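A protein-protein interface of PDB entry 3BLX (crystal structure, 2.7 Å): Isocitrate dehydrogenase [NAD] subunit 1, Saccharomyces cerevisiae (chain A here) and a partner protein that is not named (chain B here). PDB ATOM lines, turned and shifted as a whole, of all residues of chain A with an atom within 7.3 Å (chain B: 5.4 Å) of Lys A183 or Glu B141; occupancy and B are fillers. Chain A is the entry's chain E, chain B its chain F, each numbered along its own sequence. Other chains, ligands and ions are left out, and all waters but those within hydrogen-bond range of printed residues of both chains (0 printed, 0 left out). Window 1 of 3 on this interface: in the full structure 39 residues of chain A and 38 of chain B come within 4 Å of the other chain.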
ATOM      1  N   VAL A 181       3.946  -6.118 -10.667  1.00  0.00           N
ATOM      2  CA  VAL A 181       2.925  -5.362  -9.962  1.00  0.00           C
ATOM      3  C   VAL A 181       1.824  -4.972 -10.943  1.00  0.00           C
ATOM      4  O   VAL A 181       2.092  -4.356 -11.961  1.00  0.00           O
ATOM      5  CB  VAL A 181       3.518  -4.073  -9.310  1.00  0.00           C
ATOM      6  CG1 VAL A 181       2.416  -3.235  -8.672  1.00  0.00           C
ATOM      7  CG2 VAL A 181       4.581  -4.428  -8.290  1.00  0.00           C
ATOM      8  N   HIS A 182       0.584  -5.307 -10.625  1.00  0.00           N
ATOM      9  CA  HIS A 182      -0.495  -5.121 -11.581  1.00  0.00           C
ATOM     10  C   HIS A 182      -1.834  -4.969 -10.862  1.00  0.00           C
ATOM     11  O   HIS A 182      -1.911  -5.064  -9.630  1.00  0.00           O
ATOM     12  CB  HIS A 182      -0.567  -6.366 -12.426  1.00  0.00           C
ATOM     13  CG  HIS A 182      -0.836  -7.591 -11.623  1.00  0.00           C
ATOM     14  ND1 HIS A 182      -2.104  -7.950 -11.217  1.00  0.00           N
ATOM     15  CD2 HIS A 182       0.003  -8.528 -11.117  1.00  0.00           C
ATOM     16  CE1 HIS A 182      -2.035  -9.068 -10.512  1.00  0.00           C
ATOM     17  NE2 HIS A 182      -0.768  -9.440 -10.440  1.00  0.00           N
ATOM     18  N   LYS A 183      -2.889  -4.751 -11.635  1.00  0.00           N
ATOM     19  CA  LYS A 183      -4.234  -4.665 -11.088  1.00  0.00           C
ATOM     20  C   LYS A 183      -5.161  -5.643 -11.833  1.00  0.00           C
ATOM     21  O   LYS A 183      -6.232  -5.265 -12.303  1.00  0.00           O
ATOM     22  CB  LYS A 183      -4.742  -3.219 -11.201  1.00  0.00           C
ATOM     23  CG  LYS A 183      -5.717  -2.769 -10.119  1.00  0.00           C
ATOM     24  CD  LYS A 183      -5.733  -1.246 -10.015  1.00  0.00           C
ATOM     25  CE  LYS A 183      -6.710  -0.770  -8.942  1.00  0.00           C
ATOM     26  NZ  LYS A 183      -6.594  -1.550  -7.671  1.00  0.00           N
ATOM     27  N   ALA A 184      -4.745  -6.903 -11.940  1.00  0.00           N
ATOM     28  CA  ALA A 184      -5.490  -7.894 -12.725  1.00  0.00           C
ATOM     29  C   ALA A 184      -6.816  -8.330 -12.103  1.00  0.00           C
ATOM     30  O   ALA A 184      -7.636  -8.970 -12.759  1.00  0.00           O
ATOM     31  CB  ALA A 184      -4.618  -9.114 -13.015  1.00  0.00           C
ATOM     32  N   ASN A 185      -7.017  -7.999 -10.833  1.00  0.00           N
ATOM     33  CA  ASN A 185      -8.270  -8.312 -10.156  1.00  0.00           C
ATOM     34  C   ASN A 185      -9.450  -7.541 -10.763  1.00  0.00           C
ATOM     35  O   ASN A 185     -10.573  -8.047 -10.820  1.00  0.00           O
ATOM     36  CB  ASN A 185      -8.146  -8.069  -8.641  1.00  0.00           C
ATOM     37  CG  ASN A 185      -7.708  -6.644  -8.299  1.00  0.00           C
ATOM     38  OD1 ASN A 185      -7.034  -5.977  -9.092  1.00  0.00           O
ATOM     39  ND2 ASN A 185      -8.082  -6.178  -7.105  1.00  0.00           N
ATOM     40  N   ILE A 186      -9.176  -6.325 -11.235  1.00  0.00           N
ATOM     41  CA  ILE A 186     -10.188  -5.456 -11.827  1.00  0.00           C
ATOM     42  C   ILE A 186     -10.057  -5.406 -13.348  1.00  0.00           C
ATOM     43  O   ILE A 186     -11.021  -5.678 -14.075  1.00  0.00           O
ATOM     44  CB  ILE A 186     -10.070  -4.022 -11.293  1.00  0.00           C
ATOM     45  CG1 ILE A 186     -10.399  -3.985  -9.804  1.00  0.00           C
ATOM     46  CG2 ILE A 186     -10.999  -3.096 -12.047  1.00  0.00           C
ATOM     47  CD1 ILE A 186     -10.352  -2.591  -9.225  1.00  0.00           C
ATOM     48  N   MET A 187      -8.867  -5.034 -13.820  1.00  0.00           N
ATOM     49  CA  MET A 187      -8.540  -5.058 -15.252  1.00  0.00           C
ATOM     50  C   MET A 187      -8.101  -6.464 -15.633  1.00  0.00           C
ATOM     51  O   MET A 187      -6.916  -6.704 -15.837  1.00  0.00           O
ATOM     52  CB  MET A 187      -7.388  -4.082 -15.584  1.00  0.00           C
ATOM     53  CG  MET A 187      -7.462  -2.682 -14.954  1.00  0.00           C
ATOM     54  SD  MET A 187      -8.847  -1.654 -15.494  1.00  0.00           S
ATOM     55  CE  MET A 187      -8.614  -1.595 -17.264  1.00  0.00           C
ATOM     56  N   LYS A 188      -9.040  -7.395 -15.715  1.00  0.00           N
ATOM     57  CA  LYS A 188      -8.696  -8.812 -15.859  1.00  0.00           C
ATOM     58  C   LYS A 188      -8.012  -9.115 -17.200  1.00  0.00           C
ATOM     59  O   LYS A 188      -7.208 -10.043 -17.328  1.00  0.00           O
ATOM     60  CB  LYS A 188      -9.951  -9.678 -15.667  1.00  0.00           C
ATOM     61  CG  LYS A 188     -10.781  -9.266 -14.452  1.00  0.00           C
ATOM     62  CD  LYS A 188     -11.846 -10.296 -14.087  1.00  0.00           C
ATOM     63  CE  LYS A 188     -12.616  -9.859 -12.837  1.00  0.00           C
ATOM     64  NZ  LYS A 188     -13.593 -10.893 -12.352  1.00  0.00           N
ATOM     65  N   LEU A 189      -8.324  -8.308 -18.202  1.00  0.00           N
ATOM     66  CA  LEU A 189      -7.783  -8.540 -19.528  1.00  0.00           C
ATOM     67  C   LEU A 189      -6.391  -7.923 -19.699  1.00  0.00           C
ATOM     68  O   LEU A 189      -5.412  -8.630 -19.985  1.00  0.00           O
ATOM     69  CB  LEU A 189      -8.717  -7.940 -20.565  1.00  0.00           C
ATOM     70  CG  LEU A 189      -8.996  -8.844 -21.755  1.00  0.00           C
ATOM     71  CD1 LEU A 189      -9.421 -10.205 -21.226  1.00  0.00           C
ATOM     72  CD2 LEU A 189     -10.086  -8.206 -22.616  1.00  0.00           C
ATOM     73  N   GLY A 190      -6.320  -6.601 -19.522  1.00  0.00           N
ATOM     74  CA  GLY A 190      -5.102  -5.835 -19.736  1.00  0.00           C
ATOM     75  C   GLY A 190      -3.996  -6.120 -18.738  1.00  0.00           C
ATOM     76  O   GLY A 190      -2.855  -6.409 -19.120  1.00  0.00           O
ATOM     77  N   ASP A 191      -4.319  -6.030 -17.452  1.00  0.00           N
ATOM     78  CA  ASP A 191      -3.322  -6.286 -16.419  1.00  0.00           C
ATOM     79  C   ASP A 191      -3.168  -7.792 -16.199  1.00  0.00           C
ATOM     80  O   ASP A 191      -2.167  -8.246 -15.648  1.00  0.00           O
ATOM     81  CB  ASP A 191      -3.637  -5.522 -15.121  1.00  0.00           C
ATOM     82  CG  ASP A 191      -3.224  -4.038 -15.190  1.00  0.00           C
ATOM     83  OD1 ASP A 191      -3.175  -3.458 -16.309  1.00  0.00           O
ATOM     84  OD2 ASP A 191      -2.951  -3.448 -14.120  1.00  0.00           O
ATOM     85  N   GLY A 192      -4.153  -8.565 -16.655  1.00  0.00           N
ATOM     86  CA  GLY A 192      -4.017 -10.011 -16.714  1.00  0.00           C
ATOM     87  C   GLY A 192      -2.928 -10.397 -17.703  1.00  0.00           C
ATOM     88  O   GLY A 192      -2.045 -11.204 -17.409  1.00  0.00           O
ATOM     89  N   PHE A 194      -0.436  -8.570 -18.648  1.00  0.00           N
ATOM     90  CA  PHE A 194       0.813  -8.170 -18.015  1.00  0.00           C
ATOM     91  C   PHE A 194       1.376  -9.200 -17.012  1.00  0.00           C
ATOM     92  O   PHE A 194       2.516  -9.652 -17.157  1.00  0.00           O
ATOM     93  CB  PHE A 194       0.636  -6.825 -17.318  1.00  0.00           C
ATOM     94  CG  PHE A 194       1.934  -6.205 -16.897  1.00  0.00           C
ATOM     95  CD1 PHE A 194       2.678  -5.429 -17.797  1.00  0.00           C
ATOM     96  CD2 PHE A 194       2.427  -6.413 -15.613  1.00  0.00           C
ATOM     97  CE1 PHE A 194       3.888  -4.869 -17.416  1.00  0.00           C
ATOM     98  CE2 PHE A 194       3.646  -5.854 -15.225  1.00  0.00           C
ATOM     99  CZ  PHE A 194       4.381  -5.087 -16.128  1.00  0.00           C
ATOM    100  N   ARG A 195       0.590  -9.545 -15.991  1.00  0.00           N
ATOM    101  CA  ARG A 195       0.956 -10.584 -15.026  1.00  0.00           C
ATOM    102  C   ARG A 195       1.310 -11.909 -15.686  1.00  0.00           C
ATOM    103  O   ARG A 195       2.286 -12.557 -15.300  1.00  0.00           O
ATOM    104  CB  ARG A 195      -0.200 -10.832 -14.057  1.00  0.00           C
ATOM    105  CG  ARG A 195      -0.009 -12.041 -13.164  1.00  0.00           C
ATOM    106  CD  ARG A 195      -1.337 -12.508 -12.579  1.00  0.00           C
ATOM    107  NE  ARG A 195      -2.242 -12.979 -13.628  1.00  0.00           N
ATOM    108  CZ  ARG A 195      -3.577 -12.918 -13.564  1.00  0.00           C
ATOM    109  NH1 ARG A 195      -4.182 -12.401 -12.488  1.00  0.00           N
ATOM    110  NH2 ARG A 195      -4.315 -13.366 -14.587  1.00  0.00           N
ATOM    111  N   ILE A 214       1.774  -9.416  -7.511  1.00  0.00           N
ATOM    112  CA  ILE A 214       1.138  -8.761  -6.403  1.00  0.00           C
ATOM    113  C   ILE A 214       0.230  -7.687  -6.953  1.00  0.00           C
ATOM    114  O   ILE A 214       0.583  -6.970  -7.888  1.00  0.00           O
ATOM    115  CB  ILE A 214       2.193  -8.202  -5.433  1.00  0.00           C
ATOM    116  CG1 ILE A 214       1.545  -7.691  -4.139  1.00  0.00           C
ATOM    117  CG2 ILE A 214       3.073  -7.155  -6.127  1.00  0.00           C
ATOM    118  CD1 ILE A 214       2.578  -7.450  -3.041  1.00  0.00           C
ATOM    119  N   ILE A 215      -0.964  -7.616  -6.399  1.00  0.00           N
ATOM    120  CA  ILE A 215      -1.895  -6.585  -6.779  1.00  0.00           C
ATOM    121  C   ILE A 215      -1.345  -5.284  -6.259  1.00  0.00           C
ATOM    122  O   ILE A 215      -0.770  -5.238  -5.164  1.00  0.00           O
ATOM    123  CB  ILE A 215      -3.282  -6.883  -6.208  1.00  0.00           C
ATOM    124  CG1 ILE A 215      -3.741  -8.249  -6.721  1.00  0.00           C
ATOM    125  CG2 ILE A 215      -4.255  -5.822  -6.629  1.00  0.00           C
ATOM    126  CD1 ILE A 215      -4.953  -8.794  -6.017  1.00  0.00           C
ATOM    127  N   VAL A 216      -1.504  -4.228  -7.044  1.00  0.00           N
ATOM    128  CA  VAL A 216      -0.796  -2.975  -6.777  1.00  0.00           C
ATOM    129  C   VAL A 216      -1.178  -2.299  -5.448  1.00  0.00           C
ATOM    130  O   VAL A 216      -0.304  -1.777  -4.741  1.00  0.00           O
ATOM    131  CB  VAL A 216      -0.948  -1.984  -7.949  1.00  0.00           C
ATOM    132  CG1 VAL A 216      -2.421  -1.650  -8.165  1.00  0.00           C
ATOM    133  CG2 VAL A 216      -0.132  -0.732  -7.699  1.00  0.00           C
ATOM    134  N   ASP A 217      -2.467  -2.313  -5.107  1.00  0.00           N
ATOM    135  CA  ASP A 217      -2.896  -1.757  -3.816  1.00  0.00           C
ATOM    136  C   ASP A 217      -2.254  -2.481  -2.620  1.00  0.00           C
ATOM    137  O   ASP A 217      -1.781  -1.827  -1.679  1.00  0.00           O
ATOM    138  CB  ASP A 217      -4.428  -1.688  -3.686  1.00  0.00           C
ATOM    139  CG  ASP A 217      -5.129  -2.954  -4.181  1.00  0.00           C
ATOM    140  OD1 ASP A 217      -4.563  -4.064  -4.039  1.00  0.00           O
ATOM    141  OD2 ASP A 217      -6.263  -2.835  -4.707  1.00  0.00           O
ATOM    142  N   ASN A 218      -2.220  -3.817  -2.682  1.00  0.00           N
ATOM    143  CA  ASN A 218      -1.527  -4.613  -1.680  1.00  0.00           C
ATOM    144  C   ASN A 218      -0.023  -4.303  -1.669  1.00  0.00           C
ATOM    145  O   ASN A 218       0.604  -4.262  -0.614  1.00  0.00           O
ATOM    146  CB  ASN A 218      -1.801  -6.116  -1.882  1.00  0.00           C
ATOM    147  CG  ASN A 218      -1.195  -6.979  -0.774  1.00  0.00           C
ATOM    148  OD1 ASN A 218      -0.493  -7.965  -1.052  1.00  0.00           O
ATOM    149  ND2 ASN A 218      -1.449  -6.608   0.488  1.00  0.00           N
ATOM    150  N   PRO A 236       3.653  -1.538 -14.996  1.00  0.00           N
ATOM    151  CA  PRO A 236       3.203  -0.664 -16.077  1.00  0.00           C
ATOM    152  C   PRO A 236       3.510   0.790 -15.725  1.00  0.00           C
ATOM    153  O   PRO A 236       3.835   1.121 -14.586  1.00  0.00           O
ATOM    154  CB  PRO A 236       1.688  -0.880 -16.087  1.00  0.00           C
ATOM    155  CG  PRO A 236       1.489  -2.224 -15.478  1.00  0.00           C
ATOM    156  CD  PRO A 236       2.554  -2.347 -14.444  1.00  0.00           C
ATOM    157  N   TYR A 239       1.585   2.657 -12.364  1.00  0.00           N
ATOM    158  CA  TYR A 239       1.831   2.365 -10.957  1.00  0.00           C
ATOM    159  C   TYR A 239       3.275   2.618 -10.533  1.00  0.00           C
ATOM    160  O   TYR A 239       3.626   2.517  -9.366  1.00  0.00           O
ATOM    161  CB  TYR A 239       1.467   0.913 -10.630  1.00  0.00           C
ATOM    162  CG  TYR A 239       0.161   0.446 -11.235  1.00  0.00           C
ATOM    163  CD1 TYR A 239      -0.994   1.229 -11.147  1.00  0.00           C
ATOM    164  CD2 TYR A 239       0.077  -0.781 -11.890  1.00  0.00           C
ATOM    165  CE1 TYR A 239      -2.190   0.807 -11.699  1.00  0.00           C
ATOM    166  CE2 TYR A 239      -1.103  -1.210 -12.451  1.00  0.00           C
ATOM    167  CZ  TYR A 239      -2.240  -0.415 -12.355  1.00  0.00           C
ATOM    168  OH  TYR A 239      -3.421  -0.845 -12.923  1.00  0.00           O
ATOM    169  N   GLU B 139     -17.703   5.846 -11.160  1.00  0.00           N
ATOM    170  CA  GLU B 139     -17.092   5.716 -12.468  1.00  0.00           C
ATOM    171  C   GLU B 139     -15.649   5.223 -12.386  1.00  0.00           C
ATOM    172  O   GLU B 139     -15.337   4.393 -11.542  1.00  0.00           O
ATOM    173  CB  GLU B 139     -17.196   7.051 -13.201  1.00  0.00           C
ATOM    174  CG  GLU B 139     -16.638   8.216 -12.403  1.00  0.00           C
ATOM    175  CD  GLU B 139     -17.146   9.587 -12.873  1.00  0.00           C
ATOM    176  OE1 GLU B 139     -18.153   9.649 -13.619  1.00  0.00           O
ATOM    177  OE2 GLU B 139     -16.538  10.607 -12.470  1.00  0.00           O
ATOM    178  N   GLY B 140     -14.781   5.721 -13.269  1.00  0.00           N
ATOM    179  CA  GLY B 140     -13.402   5.260 -13.355  1.00  0.00           C
ATOM    180  C   GLY B 140     -13.293   3.824 -13.869  1.00  0.00           C
ATOM    181  O   GLY B 140     -14.033   3.377 -14.773  1.00  0.00           O
ATOM    182  N   GLU B 141     -12.364   3.088 -13.277  1.00  0.00           N
ATOM    183  CA  GLU B 141     -12.097   1.732 -13.711  1.00  0.00           C
ATOM    184  C   GLU B 141     -13.176   0.739 -13.277  1.00  0.00           C
ATOM    185  O   GLU B 141     -13.150  -0.429 -13.658  1.00  0.00           O
ATOM    186  CB  GLU B 141     -10.712   1.289 -13.231  1.00  0.00           C
ATOM    187  CG  GLU B 141     -10.455   1.521 -11.753  1.00  0.00           C
ATOM    188  CD  GLU B 141      -8.982   1.388 -11.390  1.00  0.00           C
ATOM    189  OE1 GLU B 141      -8.143   1.301 -12.320  1.00  0.00           O
ATOM    190  OE2 GLU B 141      -8.667   1.378 -10.174  1.00  0.00           O
ATOM    191  N   TYR B 142     -14.130   1.211 -12.485  1.00  0.00           N
ATOM    192  CA  TYR B 142     -15.260   0.388 -12.061  1.00  0.00           C
ATOM    193  C   TYR B 142     -16.313   0.283 -13.170  1.00  0.00           C
ATOM    194  O   TYR B 142     -16.837  -0.805 -13.420  1.00  0.00           O
ATOM    195  CB  TYR B 142     -15.883   0.948 -10.779  1.00  0.00           C
ATOM    196  CG  TYR B 142     -15.045   0.732  -9.528  1.00  0.00           C
ATOM    197  CD1 TYR B 142     -13.723   0.309  -9.619  1.00  0.00           C
ATOM    198  CD2 TYR B 142     -15.564   0.976  -8.256  1.00  0.00           C
ATOM    199  CE1 TYR B 142     -12.947   0.117  -8.493  1.00  0.00           C
ATOM    200  CE2 TYR B 142     -14.788   0.786  -7.117  1.00  0.00           C
ATOM    201  CZ  TYR B 142     -13.474   0.354  -7.250  1.00  0.00           C
ATOM    202  OH  TYR B 142     -12.672   0.153  -6.146  1.00  0.00           O
ATOM    203  N   SER B 143     -16.623   1.410 -13.818  1.00  0.00           N
ATOM    204  CA  SER B 143     -17.448   1.411 -15.035  1.00  0.00           C
ATOM    205  C   SER B 143     -16.608   1.258 -16.345  1.00  0.00           C
ATOM    206  O   SER B 143     -17.053   1.622 -17.455  1.00  0.00           O
ATOM    207  CB  SER B 143     -18.353   2.657 -15.078  1.00  0.00           C
ATOM    208  OG  SER B 143     -17.621   3.858 -15.284  1.00  0.00           O
ATOM    209  N   GLY B 144     -15.408   0.687 -16.194  1.00  0.00           N
ATOM    210  CA  GLY B 144     -14.474   0.498 -17.288  1.00  0.00           C
ATOM    211  C   GLY B 144     -14.766  -0.649 -18.242  1.00  0.00           C
ATOM    212  O   GLY B 144     -15.397  -1.653 -17.875  1.00  0.00           O
ATOM    213  N   LYS B 158     -12.184   4.308 -19.995  1.00  0.00           N
ATOM    214  CA  LYS B 158     -12.535   4.736 -18.638  1.00  0.00           C
ATOM    215  C   LYS B 158     -13.160   6.102 -18.740  1.00  0.00           C
ATOM    216  O   LYS B 158     -12.777   6.929 -19.574  1.00  0.00           O
ATOM    217  CB  LYS B 158     -11.318   4.811 -17.684  1.00  0.00           C
ATOM    218  CG  LYS B 158     -10.836   3.471 -17.137  1.00  0.00           C
ATOM    219  CD  LYS B 158      -9.403   3.585 -16.646  1.00  0.00           C
ATOM    220  CE  LYS B 158      -8.683   2.231 -16.634  1.00  0.00           C
ATOM    221  NZ  LYS B 158      -7.189   2.355 -16.506  1.00  0.00           N
ATOM    222  N   ASN B 244     -11.676   8.034  -8.849  1.00  0.00           N
ATOM    223  CA  ASN B 244     -11.736   6.604  -8.572  1.00  0.00           C
ATOM    224  C   ASN B 244     -10.442   5.850  -8.860  1.00  0.00           C
ATOM    225  O   ASN B 244     -10.133   4.868  -8.161  1.00  0.00           O
ATOM    226  CB  ASN B 244     -12.900   5.959  -9.316  1.00  0.00           C
ATOM    227  CG  ASN B 244     -12.892   4.438  -9.196  1.00  0.00           C
ATOM    228  OD1 ASN B 244     -12.682   3.741 -10.182  1.00  0.00           O
ATOM    229  ND2 ASN B 244     -13.102   3.919  -7.983  1.00  0.00           N
ATOM    230  N   LEU B 245      -9.705   6.317  -9.879  1.00  0.00           N
ATOM    231  CA  LEU B 245      -8.456   5.696 -10.352  1.00  0.00           C
ATOM    232  C   LEU B 245      -7.384   5.334  -9.282  1.00  0.00           C
ATOM    233  O   LEU B 245      -6.864   4.217  -9.228  1.00  0.00           O
ATOM    234  CB  LEU B 245      -7.841   6.590 -11.431  1.00  0.00           C
ATOM    235  CG  LEU B 245      -6.930   5.851 -12.409  1.00  0.00           C
ATOM    236  CD1 LEU B 245      -7.792   5.074 -13.409  1.00  0.00           C
ATOM    237  CD2 LEU B 245      -5.949   6.795 -13.130  1.00  0.00           C
ATOM    238  N   ASP B 248      -8.207   3.115  -4.757  1.00  0.00           N
ATOM    239  CA  ASP B 248      -7.792   1.811  -4.243  1.00  0.00           C
ATOM    240  C   ASP B 248      -6.389   1.862  -3.624  1.00  0.00           C
ATOM    241  O   ASP B 248      -6.196   1.526  -2.465  1.00  0.00           O
ATOM    242  CB  ASP B 248      -7.831   0.763  -5.373  1.00  0.00           C
ATOM    243  CG  ASP B 248      -9.127  -0.067  -5.382  1.00  0.00           C
ATOM    244  OD1 ASP B 248      -9.749  -0.247  -4.307  1.00  0.00           O
ATOM    245  OD2 ASP B 248      -9.517  -0.557  -6.468  1.00  0.00           O
ATOM    246  N   ILE B 249      -5.418   2.284  -4.429  1.00  0.00           N
ATOM    247  CA  ILE B 249      -4.007   2.325  -4.054  1.00  0.00           C
ATOM    248  C   ILE B 249      -3.728   3.212  -2.820  1.00  0.00           C
ATOM    249  O   ILE B 249      -3.081   2.774  -1.854  1.00  0.00           O
ATOM    250  CB  ILE B 249      -3.176   2.841  -5.249  1.00  0.00           C
ATOM    251  CG1 ILE B 249      -3.363   1.914  -6.446  1.00  0.00           C
ATOM    252  CG2 ILE B 249      -1.710   2.977  -4.892  1.00  0.00           C
ATOM    253  CD1 ILE B 249      -2.975   2.546  -7.766  1.00  0.00           C
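The side-chain amino group of Lys A183 is in salt-bridge range of the side-chain carboxylate of Asp B248, 3.3 Å away.
OD2 of Asp A217 lies within salt-bridge range of NZ of Lys A183 (3.2 Å). The side-chain carboxylate (OD2) of Asp A191 lies within hydrogen-bond range of the backbone NH (N) of Lys A183. The backbone carbonyl oxygen (O) of Met A187 is in hydrogen-bond range of the backbone NH (N) of Gly A192. The backbone carbonyl oxygen (O) of Lys A183 lies close to the side-chain amide oxygen (OD1) of Asn A185 (3.4 Å). OH of Tyr B142 sits at hydrogen-bond distance from OD2 of Asp B248 (3.2 Å). OD1 of Asn B244 lies within hydrogen-bond range of N of Glu B141.
Among the printed residues, merely in contact across the chains: Lys A183 with Glu B141, Ile A186 with Glu B141, Ile A186 with Tyr B142, Ile A186 with Asp B248, Met A187 with Lys B158 and Asp A217 with Asp B248.
Of chain B, only Glu B141 and Asp B248 come within 4 Å of Lys A183. Of the printed residues of chain B, Ile A186 touches Glu B141, Tyr B142 and Asp B248. Printed residues of chain B within 4 Å of Met A187: Lys B158 (3.9 Å). Asp A191 touches none of the printed residues of chain B. Printed residues of chain B within 4 Å of Asp A217: Asp B248 (3.9 Å). Glu B141 touches just these residues of chain A: Lys A183 and Ile A186. Of the printed residues of chain A, Tyr B142 touches Ile A186. Printed residues of chain A within 4 Å of Asp B248: Lys A183 (3.3 Å), Ile A186 (3.5 Å) and Asp A217 (3.9 Å). Ile B249 touches none of the printed residues of chain A. The nearest printed residue of chain A that does not touch Asp B248 is Asn A185 (5.8 Å).
Printed residues of chain A that touch a printed residue of chain B: Lys A183, Ile A186, Met A187 and Asp A217. Hydrophobic or aromatic side chains of chain A within 4 Å of the printed part of chain B: Ile A186 and Met A187. Along chain A the printed residues that touch a printed residue of chain B span positions 183 to 217. Printed residues of chain B that touch a printed residue of chain A: Glu B141, Tyr B142, Lys B158 and Asp B248. Hydrophobic or aromatic side chains of chain B that line the printed part of chain A: Tyr B142. Among the printed residues, Asp or Glu carboxylates within 4 Å of a Lys or Arg side-chain nitrogen of the other chain: Lys A183 with Asp B248.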
